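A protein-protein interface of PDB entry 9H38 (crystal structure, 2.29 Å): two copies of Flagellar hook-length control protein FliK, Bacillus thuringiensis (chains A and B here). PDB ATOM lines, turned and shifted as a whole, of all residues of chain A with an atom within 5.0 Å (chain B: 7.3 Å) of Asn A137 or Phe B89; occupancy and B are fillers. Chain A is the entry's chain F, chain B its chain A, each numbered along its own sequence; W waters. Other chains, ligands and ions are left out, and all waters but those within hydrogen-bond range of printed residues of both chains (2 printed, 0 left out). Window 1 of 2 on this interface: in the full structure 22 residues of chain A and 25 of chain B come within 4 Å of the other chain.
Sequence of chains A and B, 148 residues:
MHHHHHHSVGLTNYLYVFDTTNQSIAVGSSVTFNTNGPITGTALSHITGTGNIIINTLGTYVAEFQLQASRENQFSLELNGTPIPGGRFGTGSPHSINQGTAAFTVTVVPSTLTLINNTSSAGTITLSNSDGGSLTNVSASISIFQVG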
ATOM      1  N   TYR A  16     -17.453   7.371   1.552  1.00  0.00           N
ATOM      2  CA  TYR A  16     -17.875   6.885   2.857  1.00  0.00           C
ATOM      3  C   TYR A  16     -18.839   5.725   2.654  1.00  0.00           C
ATOM      4  O   TYR A  16     -19.811   5.857   1.904  1.00  0.00           O
ATOM      5  CB  TYR A  16     -18.544   8.000   3.666  1.00  0.00           C
ATOM      6  CG  TYR A  16     -19.051   7.585   5.034  1.00  0.00           C
ATOM      7  CD1 TYR A  16     -18.244   6.877   5.904  1.00  0.00           C
ATOM      8  CD2 TYR A  16     -20.338   7.893   5.447  1.00  0.00           C
ATOM      9  CE1 TYR A  16     -18.688   6.496   7.151  1.00  0.00           C
ATOM     10  CE2 TYR A  16     -20.796   7.504   6.692  1.00  0.00           C
ATOM     11  CZ  TYR A  16     -19.958   6.802   7.538  1.00  0.00           C
ATOM     12  OH  TYR A  16     -20.383   6.403   8.793  1.00  0.00           O
ATOM     13  N   ASP A  19     -22.150   0.140   7.561  1.00  0.00           N
ATOM     14  CA  ASP A  19     -23.095  -0.933   7.782  1.00  0.00           C
ATOM     15  C   ASP A  19     -23.899  -0.669   9.041  1.00  0.00           C
ATOM     16  O   ASP A  19     -23.363  -0.142  10.027  1.00  0.00           O
ATOM     17  CB  ASP A  19     -22.392  -2.281   7.931  1.00  0.00           C
ATOM     18  CG  ASP A  19     -23.327  -3.436   7.715  1.00  0.00           C
ATOM     19  OD1 ASP A  19     -23.844  -3.564   6.571  1.00  0.00           O
ATOM     20  OD2 ASP A  19     -23.550  -4.203   8.682  1.00  0.00           O
ATOM     21  N   THR A  20     -25.179  -1.094   9.023  1.00  0.00           N
ATOM     22  CA  THR A  20     -26.064  -0.960  10.177  1.00  0.00           C
ATOM     23  C   THR A  20     -26.648  -2.298  10.634  1.00  0.00           C
ATOM     24  O   THR A  20     -27.771  -2.333  11.148  1.00  0.00           O
ATOM     25  CB  THR A  20     -27.208   0.030   9.893  1.00  0.00           C
ATOM     26  OG1 THR A  20     -28.079  -0.482   8.873  1.00  0.00           O
ATOM     27  CG2 THR A  20     -26.679   1.375   9.445  1.00  0.00           C
ATOM     28  N   GLN A  66     -13.850   1.742  11.343  1.00  0.00           N
ATOM     29  CA  GLN A  66     -14.460   1.581  12.651  1.00  0.00           C
ATOM     30  C   GLN A  66     -15.335   0.339  12.588  1.00  0.00           C
ATOM     31  O   GLN A  66     -15.970   0.074  11.565  1.00  0.00           O
ATOM     32  CB  GLN A  66     -15.315   2.805  13.037  1.00  0.00           C
ATOM     33  CG  GLN A  66     -16.438   2.504  14.061  1.00  0.00           C
ATOM     34  CD  GLN A  66     -17.748   2.002  13.426  1.00  0.00           C
ATOM     35  OE1 GLN A  66     -17.980   2.169  12.228  1.00  0.00           O
ATOM     36  NE2 GLN A  66     -18.599   1.384  14.237  1.00  0.00           N
ATOM     37  N   SER A 128     -22.197  -5.569  16.293  1.00  0.00           N
ATOM     38  CA  SER A 128     -23.331  -5.069  17.055  1.00  0.00           C
ATOM     39  C   SER A 128     -23.687  -3.667  16.581  1.00  0.00           C
ATOM     40  O   SER A 128     -22.828  -2.777  16.566  1.00  0.00           O
ATOM     41  CB  SER A 128     -23.026  -5.049  18.564  1.00  0.00           C
ATOM     42  OG  SER A 128     -23.997  -4.279  19.265  1.00  0.00           O
ATOM     43  N   ASN A 129     -24.950  -3.477  16.209  1.00  0.00           N
ATOM     44  CA  ASN A 129     -25.502  -2.179  15.870  1.00  0.00           C
ATOM     45  C   ASN A 129     -26.324  -1.597  17.008  1.00  0.00           C
ATOM     46  O   ASN A 129     -27.198  -0.756  16.767  1.00  0.00           O
ATOM     47  CB  ASN A 129     -26.370  -2.293  14.614  1.00  0.00           C
ATOM     48  CG  ASN A 129     -27.609  -3.156  14.852  1.00  0.00           C
ATOM     49  OD1 ASN A 129     -27.809  -3.677  15.955  1.00  0.00           O
ATOM     50  ND2 ASN A 129     -28.447  -3.295  13.830  1.00  0.00           N
ATOM     51  N   SER A 130     -26.091  -2.047  18.239  1.00  0.00           N
ATOM     52  CA  SER A 130     -27.011  -1.738  19.320  1.00  0.00           C
ATOM     53  C   SER A 130     -26.307  -1.274  20.577  1.00  0.00           C
ATOM     54  O   SER A 130     -26.978  -0.995  21.578  1.00  0.00           O
ATOM     55  CB  SER A 130     -27.888  -2.961  19.654  1.00  0.00           C
ATOM     56  OG  SER A 130     -27.111  -4.029  20.165  1.00  0.00           O
ATOM     57  N   ASP A 131     -24.990  -1.167  20.552  1.00  0.00           N
ATOM     58  CA  ASP A 131     -24.259  -0.860  21.768  1.00  0.00           C
ATOM     59  C   ASP A 131     -24.636   0.510  22.309  1.00  0.00           C
ATOM     60  O   ASP A 131     -24.825   1.467  21.551  1.00  0.00           O
ATOM     61  CB  ASP A 131     -22.756  -0.929  21.509  1.00  0.00           C
ATOM     62  CG  ASP A 131     -22.230  -2.334  21.605  1.00  0.00           C
ATOM     63  OD1 ASP A 131     -23.024  -3.281  21.441  1.00  0.00           O
ATOM     64  OD2 ASP A 131     -21.027  -2.494  21.871  1.00  0.00           O
ATOM     65  N   LEU A 135     -31.152   2.899  19.911  1.00  0.00           N
ATOM     66  CA  LEU A 135     -31.293   3.229  18.502  1.00  0.00           C
ATOM     67  C   LEU A 135     -30.225   2.479  17.728  1.00  0.00           C
ATOM     68  O   LEU A 135     -29.313   1.902  18.316  1.00  0.00           O
ATOM     69  CB  LEU A 135     -31.186   4.746  18.275  1.00  0.00           C
ATOM     70  CG  LEU A 135     -32.286   5.660  18.839  1.00  0.00           C
ATOM     71  CD1 LEU A 135     -32.026   7.103  18.473  1.00  0.00           C
ATOM     72  CD2 LEU A 135     -33.670   5.258  18.347  1.00  0.00           C
ATOM     73  N   THR A 136     -30.343   2.500  16.402  1.00  0.00           N
ATOM     74  CA  THR A 136     -29.464   1.725  15.533  1.00  0.00           C
ATOM     75  C   THR A 136     -28.145   2.462  15.296  1.00  0.00           C
ATOM     76  O   THR A 136     -28.142   3.627  14.886  1.00  0.00           O
ATOM     77  CB  THR A 136     -30.168   1.456  14.203  1.00  0.00           C
ATOM     78  OG1 THR A 136     -31.438   0.853  14.460  1.00  0.00           O
ATOM     79  CG2 THR A 136     -29.357   0.503  13.330  1.00  0.00           C
ATOM     80  N   ASN A 137     -27.028   1.776  15.537  1.00  0.00           N
ATOM     81  CA  ASN A 137     -25.696   2.313  15.275  1.00  0.00           C
ATOM     82  C   ASN A 137     -25.170   1.917  13.899  1.00  0.00           C
ATOM     83  O   ASN A 137     -25.607   0.943  13.272  1.00  0.00           O
ATOM     84  CB  ASN A 137     -24.691   1.820  16.305  1.00  0.00           C
ATOM     85  CG  ASN A 137     -24.948   2.382  17.689  1.00  0.00           C
ATOM     86  OD1 ASN A 137     -25.181   3.598  17.852  1.00  0.00           O
ATOM     87  ND2 ASN A 137     -24.914   1.505  18.695  1.00  0.00           N
ATOM     88  N   VAL A 138     -24.206   2.699  13.434  1.00  0.00           N
ATOM     89  CA  VAL A 138     -23.246   2.177  12.481  1.00  0.00           C
ATOM     90  C   VAL A 138     -22.444   1.095  13.186  1.00  0.00           C
ATOM     91  O   VAL A 138     -21.799   1.346  14.215  1.00  0.00           O
ATOM     92  CB  VAL A 138     -22.338   3.289  11.966  1.00  0.00           C
ATOM     93  CG1 VAL A 138     -21.291   2.714  11.037  1.00  0.00           C
ATOM     94  CG2 VAL A 138     -23.176   4.375  11.299  1.00  0.00           C
ATOM     95  N   SER A 139     -22.518  -0.117  12.667  1.00  0.00           N
ATOM     96  CA  SER A 139     -21.757  -1.223  13.225  1.00  0.00           C
ATOM     97  C   SER A 139     -20.374  -1.338  12.598  1.00  0.00           C
ATOM     98  O   SER A 139     -19.450  -1.827  13.252  1.00  0.00           O
ATOM     99  CB  SER A 139     -22.539  -2.533  13.063  1.00  0.00           C
ATOM    100  OG  SER A 139     -22.833  -2.785  11.693  1.00  0.00           O
ATOM    101  N   SER A 141     -17.714   0.813   9.426  1.00  0.00           N
ATOM    102  CA  SER A 141     -17.640   1.862   8.415  1.00  0.00           C
ATOM    103  C   SER A 141     -16.208   2.016   7.914  1.00  0.00           C
ATOM    104  O   SER A 141     -15.244   1.686   8.622  1.00  0.00           O
ATOM    105  CB  SER A 141     -18.152   3.190   8.979  1.00  0.00           C
ATOM    106  OG  SER A 141     -17.484   3.506  10.189  1.00  0.00           O
ATOM    107  N   ALA B  63     -17.068  14.567   8.905  1.00  0.00           N
ATOM    108  CA  ALA B  63     -17.024  14.932  10.316  1.00  0.00           C
ATOM    109  C   ALA B  63     -16.568  13.748  11.165  1.00  0.00           C
ATOM    110  O   ALA B  63     -17.195  12.675  11.156  1.00  0.00           O
ATOM    111  CB  ALA B  63     -18.387  15.431  10.794  1.00  0.00           C
ATOM    112  N   PHE B  65     -15.827  12.657  15.165  1.00  0.00           N
ATOM    113  CA  PHE B  65     -15.992  13.014  16.566  1.00  0.00           C
ATOM    114  C   PHE B  65     -15.418  11.941  17.467  1.00  0.00           C
ATOM    115  O   PHE B  65     -15.365  10.757  17.111  1.00  0.00           O
ATOM    116  CB  PHE B  65     -17.457  13.262  16.963  1.00  0.00           C
ATOM    117  CG  PHE B  65     -18.280  12.005  17.169  1.00  0.00           C
ATOM    118  CD1 PHE B  65     -18.320  11.373  18.399  1.00  0.00           C
ATOM    119  CD2 PHE B  65     -19.072  11.504  16.144  1.00  0.00           C
ATOM    120  CE1 PHE B  65     -19.098  10.240  18.588  1.00  0.00           C
ATOM    121  CE2 PHE B  65     -19.857  10.381  16.321  1.00  0.00           C
ATOM    122  CZ  PHE B  65     -19.876   9.748  17.543  1.00  0.00           C
ATOM    123  N   ASN B  73     -22.573   4.542  25.956  1.00  0.00           N
ATOM    124  CA  ASN B  73     -23.383   5.656  25.474  1.00  0.00           C
ATOM    125  C   ASN B  73     -23.547   5.544  23.967  1.00  0.00           C
ATOM    126  O   ASN B  73     -22.825   4.799  23.294  1.00  0.00           O
ATOM    127  CB  ASN B  73     -22.753   7.006  25.833  1.00  0.00           C
ATOM    128  CG  ASN B  73     -21.356   7.162  25.248  1.00  0.00           C
ATOM    129  OD1 ASN B  73     -21.187   7.424  24.048  1.00  0.00           O
ATOM    130  ND2 ASN B  73     -20.347   6.969  26.084  1.00  0.00           N
ATOM    131  N   GLN B  74     -24.497   6.335  23.452  1.00  0.00           N
ATOM    132  CA  GLN B  74     -24.908   6.331  22.047  1.00  0.00           C
ATOM    133  C   GLN B  74     -25.178   7.768  21.623  1.00  0.00           C
ATOM    134  O   GLN B  74     -26.148   8.389  22.078  1.00  0.00           O
ATOM    135  CB  GLN B  74     -26.150   5.471  21.830  1.00  0.00           C
ATOM    136  CG  GLN B  74     -26.699   5.556  20.413  1.00  0.00           C
ATOM    137  CD  GLN B  74     -27.832   4.564  20.137  1.00  0.00           C
ATOM    138  OE1 GLN B  74     -29.011   4.803  20.479  1.00  0.00           O
ATOM    139  NE2 GLN B  74     -27.483   3.445  19.504  1.00  0.00           N
ATOM    140  N   PHE B  75     -24.322   8.292  20.759  1.00  0.00           N
ATOM    141  CA  PHE B  75     -24.448   9.639  20.226  1.00  0.00           C
ATOM    142  C   PHE B  75     -24.526   9.582  18.709  1.00  0.00           C
ATOM    143  O   PHE B  75     -23.974   8.681  18.075  1.00  0.00           O
ATOM    144  CB  PHE B  75     -23.268  10.522  20.639  1.00  0.00           C
ATOM    145  CG  PHE B  75     -23.328  10.970  22.055  1.00  0.00           C
ATOM    146  CD1 PHE B  75     -23.035  10.087  23.089  1.00  0.00           C
ATOM    147  CD2 PHE B  75     -23.674  12.277  22.364  1.00  0.00           C
ATOM    148  CE1 PHE B  75     -23.076  10.500  24.391  1.00  0.00           C
ATOM    149  CE2 PHE B  75     -23.737  12.704  23.676  1.00  0.00           C
ATOM    150  CZ  PHE B  75     -23.444  11.819  24.696  1.00  0.00           C
ATOM    151  N   SER B  76     -25.213  10.559  18.138  1.00  0.00           N
ATOM    152  CA  SER B  76     -25.337  10.667  16.698  1.00  0.00           C
ATOM    153  C   SER B  76     -25.000  12.080  16.268  1.00  0.00           C
ATOM    154  O   SER B  76     -25.364  13.042  16.944  1.00  0.00           O
ATOM    155  CB  SER B  76     -26.756  10.315  16.219  1.00  0.00           C
ATOM    156  OG  SER B  76     -26.833  10.345  14.793  1.00  0.00           O
ATOM    157  N   LEU B  77     -24.310  12.200  15.142  1.00  0.00           N
ATOM    158  CA  LEU B  77     -24.260  13.470  14.438  1.00  0.00           C
ATOM    159  C   LEU B  77     -25.640  13.787  13.879  1.00  0.00           C
ATOM    160  O   LEU B  77     -26.338  12.901  13.378  1.00  0.00           O
ATOM    161  CB  LEU B  77     -23.240  13.412  13.305  1.00  0.00           C
ATOM    162  CG  LEU B  77     -21.804  13.196  13.774  1.00  0.00           C
ATOM    163  CD1 LEU B  77     -20.913  12.819  12.593  1.00  0.00           C
ATOM    164  CD2 LEU B  77     -21.281  14.446  14.493  1.00  0.00           C
ATOM    165  N   GLY B  86     -25.845   7.130   8.804  1.00  0.00           N
ATOM    166  CA  GLY B  86     -24.478   6.738   9.067  1.00  0.00           C
ATOM    167  C   GLY B  86     -23.764   7.604  10.076  1.00  0.00           C
ATOM    168  O   GLY B  86     -22.535   7.645  10.086  1.00  0.00           O
ATOM    169  N   GLY B  87     -24.497   8.285  10.936  1.00  0.00           N
ATOM    170  CA  GLY B  87     -23.845   9.171  11.872  1.00  0.00           C
ATOM    171  C   GLY B  87     -24.025   8.820  13.334  1.00  0.00           C
ATOM    172  O   GLY B  87     -23.649   9.618  14.200  1.00  0.00           O
ATOM    173  N   ARG B  88     -24.581   7.656  13.649  1.00  0.00           N
ATOM    174  CA  ARG B  88     -24.838   7.280  15.037  1.00  0.00           C
ATOM    175  C   ARG B  88     -23.871   6.185  15.467  1.00  0.00           C
ATOM    176  O   ARG B  88     -23.709   5.184  14.764  1.00  0.00           O
ATOM    177  CB  ARG B  88     -26.285   6.823  15.245  1.00  0.00           C
ATOM    178  CG  ARG B  88     -26.618   6.624  16.733  1.00  0.00           C
ATOM    179  CD  ARG B  88     -28.046   6.134  16.963  1.00  0.00           C
ATOM    180  NE  ARG B  88     -29.028   7.133  16.544  1.00  0.00           N
ATOM    181  CZ  ARG B  88     -29.821   6.991  15.490  1.00  0.00           C
ATOM    182  NH1 ARG B  88     -29.813   5.881  14.769  1.00  0.00           N
ATOM    183  NH2 ARG B  88     -30.635   7.988  15.149  1.00  0.00           N
ATOM    184  N   PHE B  89     -23.225   6.383  16.620  1.00  0.00           N
ATOM    185  CA  PHE B  89     -22.191   5.468  17.098  1.00  0.00           C
ATOM    186  C   PHE B  89     -22.361   5.214  18.595  1.00  0.00           C
ATOM    187  O   PHE B  89     -22.711   6.121  19.353  1.00  0.00           O
ATOM    188  CB  PHE B  89     -20.775   6.023  16.812  1.00  0.00           C
ATOM    189  CG  PHE B  89     -20.435   6.096  15.345  1.00  0.00           C
ATOM    190  CD1 PHE B  89     -20.906   7.124  14.561  1.00  0.00           C
ATOM    191  CD2 PHE B  89     -19.665   5.116  14.751  1.00  0.00           C
ATOM    192  CE1 PHE B  89     -20.595   7.188  13.209  1.00  0.00           C
ATOM    193  CE2 PHE B  89     -19.356   5.175  13.379  1.00  0.00           C
ATOM    194  CZ  PHE B  89     -19.817   6.210  12.625  1.00  0.00           C
ATOM    195  N   GLY B  90     -22.112   3.980  19.012  1.00  0.00           N
ATOM    196  CA  GLY B  90     -22.272   3.607  20.404  1.00  0.00           C
ATOM    197  C   GLY B  90     -21.176   2.662  20.840  1.00  0.00           C
ATOM    198  O   GLY B  90     -20.665   1.849  20.057  1.00  0.00           O
ATOM    199  N   THR B  91     -20.807   2.771  22.109  1.00  0.00           N
ATOM    200  CA  THR B  91     -19.893   1.797  22.676  1.00  0.00           C
ATOM    201  C   THR B  91     -20.583   1.128  23.851  1.00  0.00           C
ATOM    202  O   THR B  91     -21.509   1.689  24.451  1.00  0.00           O
ATOM    203  CB  THR B  91     -18.557   2.423  23.122  1.00  0.00           C
ATOM    204  OG1 THR B  91     -17.852   1.485  23.942  1.00  0.00           O
ATOM    205  CG2 THR B  91     -18.782   3.702  23.931  1.00  0.00           C
ATOM    206  N   ASN B  98     -15.920   6.660  22.507  1.00  0.00           N
ATOM    207  CA  ASN B  98     -16.902   6.577  21.435  1.00  0.00           C
ATOM    208  C   ASN B  98     -16.386   7.419  20.270  1.00  0.00           C
ATOM    209  O   ASN B  98     -16.239   8.642  20.394  1.00  0.00           O
ATOM    210  CB  ASN B  98     -18.287   7.042  21.894  1.00  0.00           C
ATOM    211  CG  ASN B  98     -19.380   6.646  20.921  1.00  0.00           C
ATOM    212  OD1 ASN B  98     -19.102   6.082  19.864  1.00  0.00           O
ATOM    213  ND2 ASN B  98     -20.628   6.959  21.255  1.00  0.00           N
ATOM    214  N   GLN B  99     -16.083   6.760  19.154  1.00  0.00           N
ATOM    215  CA  GLN B  99     -15.432   7.415  18.032  1.00  0.00           C
ATOM    216  C   GLN B  99     -16.198   7.094  16.761  1.00  0.00           C
ATOM    217  O   GLN B  99     -16.449   5.920  16.465  1.00  0.00           O
ATOM    218  CB  GLN B  99     -13.962   6.974  17.918  1.00  0.00           C
ATOM    219  CG  GLN B  99     -13.062   7.955  17.201  1.00  0.00           C
ATOM    220  CD  GLN B  99     -13.158   7.833  15.676  1.00  0.00           C
ATOM    221  OE1 GLN B  99     -13.235   6.735  15.146  1.00  0.00           O
ATOM    222  NE2 GLN B  99     -13.161   8.966  14.976  1.00  0.00           N
ATOM    223  N   GLY B 100     -16.578   8.139  16.020  1.00  0.00           N
ATOM    224  CA  GLY B 100     -17.277   7.968  14.759  1.00  0.00           C
ATOM    225  C   GLY B 100     -16.831   8.927  13.668  1.00  0.00           C
ATOM    226  O   GLY B 100     -16.617  10.116  13.939  1.00  0.00           O
ATOM    227  N   THR B 101     -16.676   8.418  12.441  1.00  0.00           N
ATOM    228  CA  THR B 101     -16.341   9.218  11.265  1.00  0.00           C
ATOM    229  C   THR B 101     -17.477   9.040  10.269  1.00  0.00           C
ATOM    230  O   THR B 101     -17.783   7.908   9.888  1.00  0.00           O
ATOM    231  CB  THR B 101     -15.009   8.787  10.627  1.00  0.00           C
ATOM    232  OG1 THR B 101     -13.925   8.836  11.575  1.00  0.00           O
ATOM    233  CG2 THR B 101     -14.673   9.681   9.458  1.00  0.00           C
ATOM    234  N   ALA B 102     -18.126  10.146   9.880  1.00  0.00           N
ATOM    235  CA  ALA B 102     -19.221  10.112   8.915  1.00  0.00           C
ATOM    236  C   ALA B 102     -19.117  11.298   7.968  1.00  0.00           C
ATOM    237  O   ALA B 102     -18.573  12.342   8.330  1.00  0.00           O
ATOM    238  CB  ALA B 102     -20.597  10.152   9.589  1.00  0.00           C
ATOM    239  N   LEU B 115     -23.924  17.194  17.870  1.00  0.00           N
ATOM    240  CA  LEU B 115     -23.604  15.845  18.311  1.00  0.00           C
ATOM    241  C   LEU B 115     -24.425  15.561  19.559  1.00  0.00           C
ATOM    242  O   LEU B 115     -24.226  16.211  20.593  1.00  0.00           O
ATOM    243  CB  LEU B 115     -22.106  15.714  18.607  1.00  0.00           C
ATOM    244  CG  LEU B 115     -21.683  14.322  19.081  1.00  0.00           C
ATOM    245  CD1 LEU B 115     -22.008  13.282  18.007  1.00  0.00           C
ATOM    246  CD2 LEU B 115     -20.193  14.299  19.476  1.00  0.00           C
ATOM    247  N   ILE B 116     -25.341  14.596  19.487  1.00  0.00           N
ATOM    248  CA  ILE B 116     -26.468  14.584  20.417  1.00  0.00           C
ATOM    249  C   ILE B 116     -26.641  13.219  21.059  1.00  0.00           C
ATOM    250  O   ILE B 116     -26.527  12.189  20.392  1.00  0.00           O
ATOM    251  CB  ILE B 116     -27.772  15.037  19.719  1.00  0.00           C
ATOM    252  CG1 ILE B 116     -27.714  16.547  19.431  1.00  0.00           C
ATOM    253  CG2 ILE B 116     -29.001  14.672  20.563  1.00  0.00           C
ATOM    254  CD1 ILE B 116     -29.018  17.135  18.813  1.00  0.00           C
ATOM    255  N   ASN B 118     -28.335  10.670  21.509  1.00  0.00           N
ATOM    256  CA  ASN B 118     -29.405  10.042  20.736  1.00  0.00           C
ATOM    257  C   ASN B 118     -29.669   8.668  21.334  1.00  0.00           C
ATOM    258  O   ASN B 118     -29.457   7.591  20.760  1.00  0.00           O
ATOM    259  CB  ASN B 118     -29.026   9.964  19.266  1.00  0.00           C
ATOM    260  CG  ASN B 118     -30.214  10.069  18.352  1.00  0.00           C
ATOM    261  OD1 ASN B 118     -31.325  10.341  18.782  1.00  0.00           O
ATOM    262  ND2 ASN B 118     -29.983   9.852  17.072  1.00  0.00           N
ATOM    263  N   SER B 120     -28.614   7.122  24.668  1.00  0.00           N
ATOM    264  CA  SER B 120     -27.911   6.171  25.505  1.00  0.00           C
ATOM    265  C   SER B 120     -28.901   5.558  26.484  1.00  0.00           C
ATOM    266  O   SER B 120     -29.795   6.241  26.991  1.00  0.00           O
ATOM    267  CB  SER B 120     -26.777   6.878  26.251  1.00  0.00           C
ATOM    268  OG  SER B 120     -26.096   7.784  25.402  1.00  0.00           O
HETATM  269  O   HOH W   1     -21.447   1.578  16.988  1.00  0.00           O
HETATM  270  O   HOH W   2     -18.720   1.730  17.371  1.00  0.00           O
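Asn A137 touches just these residues of chain B: Gln B74, Arg B88, Phe B89 and Gly B90. Phe B89 touches just these residues of chain A: Tyr A16 (3.9 Å), Gln A66 (3.5 Å), Asn A137 (3.3 Å) and Val A138 (3.8 Å). Of the printed residues of chain B, Tyr A16 touches Gly B86 (2.8 Å), Phe B89 (3.9 Å), Thr B101 (3.2 Å) and Ala B102 (3.7 Å). Of the printed residues of chain B, Thr A136 touches Arg B88. Phe B75 touches none of the printed residues of chain A. Ser A139 touches none of the printed residues of chain B. The nearest residue of chain A that does not touch Phe B89 is Ser A141 (4.1 Å).
O of Gly B86 lies within hydrogen-bond range of OH of Tyr A16 (2.8 Å). N of Gly B90 sits at hydrogen-bond distance from OD1 of Asn A137. The backbone carbonyl oxygen (O) of Thr B101 lies within hydrogen-bond range of the side-chain hydroxyl (OH) of Tyr A16 (3.2 Å). O of Leu A135 sits at hydrogen-bond distance from NE2 of Gln B74. The backbone carbonyl oxygen (O) of Arg B88 sits at hydrogen-bond distance from the backbone NH (N) of Val A138 (2.9 Å). NH1 of Arg B88 sits at hydrogen-bond distance from O of Thr A136 (2.8 Å). The side-chain amide nitrogen (NE2) of Gln B74 sits at hydrogen-bond distance from the side-chain amide oxygen (OD1) of Asn A137, at 2.8 Å.
The backbone carbonyl oxygen of Phe B75 sits at hydrogen-bond distance from the backbone NH of Phe B89, 2.8 Å away. The side-chain amide nitrogen (ND2) of Asn A137 sits at hydrogen-bond distance from the backbone carbonyl oxygen (O) of Asp A131, 2.9 Å away. The side-chain amide nitrogen (NE2) of Gln B99 lies within hydrogen-bond range of the side-chain hydroxyl (OG1) of Thr B101 (3.5 Å). N of Ala B63 is in hydrogen-bond range of O of Ala B102. O of Asn A129 sits at hydrogen-bond distance from N of Asn A137 (2.8 Å). The side-chain amide nitrogen of Gln A66 lies within hydrogen-bond range of the backbone carbonyl oxygen of Val A138.
No position is printed for both chains. Of the 19 pairs that touch across the chains among the printed residues, none has its exchanged pair printed and touching as well.
Phe B89 touches Tyr A16 (CZ to OH, 3.9 Å). Ala B102 touches Tyr A16. Phe B89 touches Gln A66 (CE2 to OE1, 3.5 Å). NE2 of Gln B74 touches O of Asp A131, at 3.9 Å. O of Asp A131 touches CA of Gly B90 (3.5 Å). Asp A131 touches Thr B91 (CB to C, 3.8 Å). CD1 of Leu A135 touches NE of Arg B88, 3.6 Å away. Leu A135 touches Asn B118 (CD1 to OD1, 3.3 Å). Asn A137 touches Arg B88 (CA to O, 3.5 Å). CB of Val A138 touches CE2 of Phe B89, at 3.8 Å.
Hydrophobic or aromatic side chains of chain B that line the printed part of chain A: Phe B89 and Ala B102. Along chain B the printed residues that touch a printed residue of chain A span positions 74 to 118. Of the 14 printed residues of chain A, 7 touch a printed residue of chain B. Hydrophobic or aromatic side chains of chain A that line the printed part of chain B: Tyr A16, Leu A135 and Val A138. Among the printed residues, 19 pairs touch across the chains. Among the printed residues, no Asp or Glu carboxylate lies within 4 Å of a Lys or Arg side-chain nitrogen of the other chain.
Water W1 lies within hydrogen-bond range of O of Val A138 (2.8 Å) and O of Gly B90 (3.2 Å). Water W2 bridges the side-chain amide nitrogen of Gln A66 (3.2 Å) and the backbone carbonyl oxygen of Gly B90 (3.3 Å).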
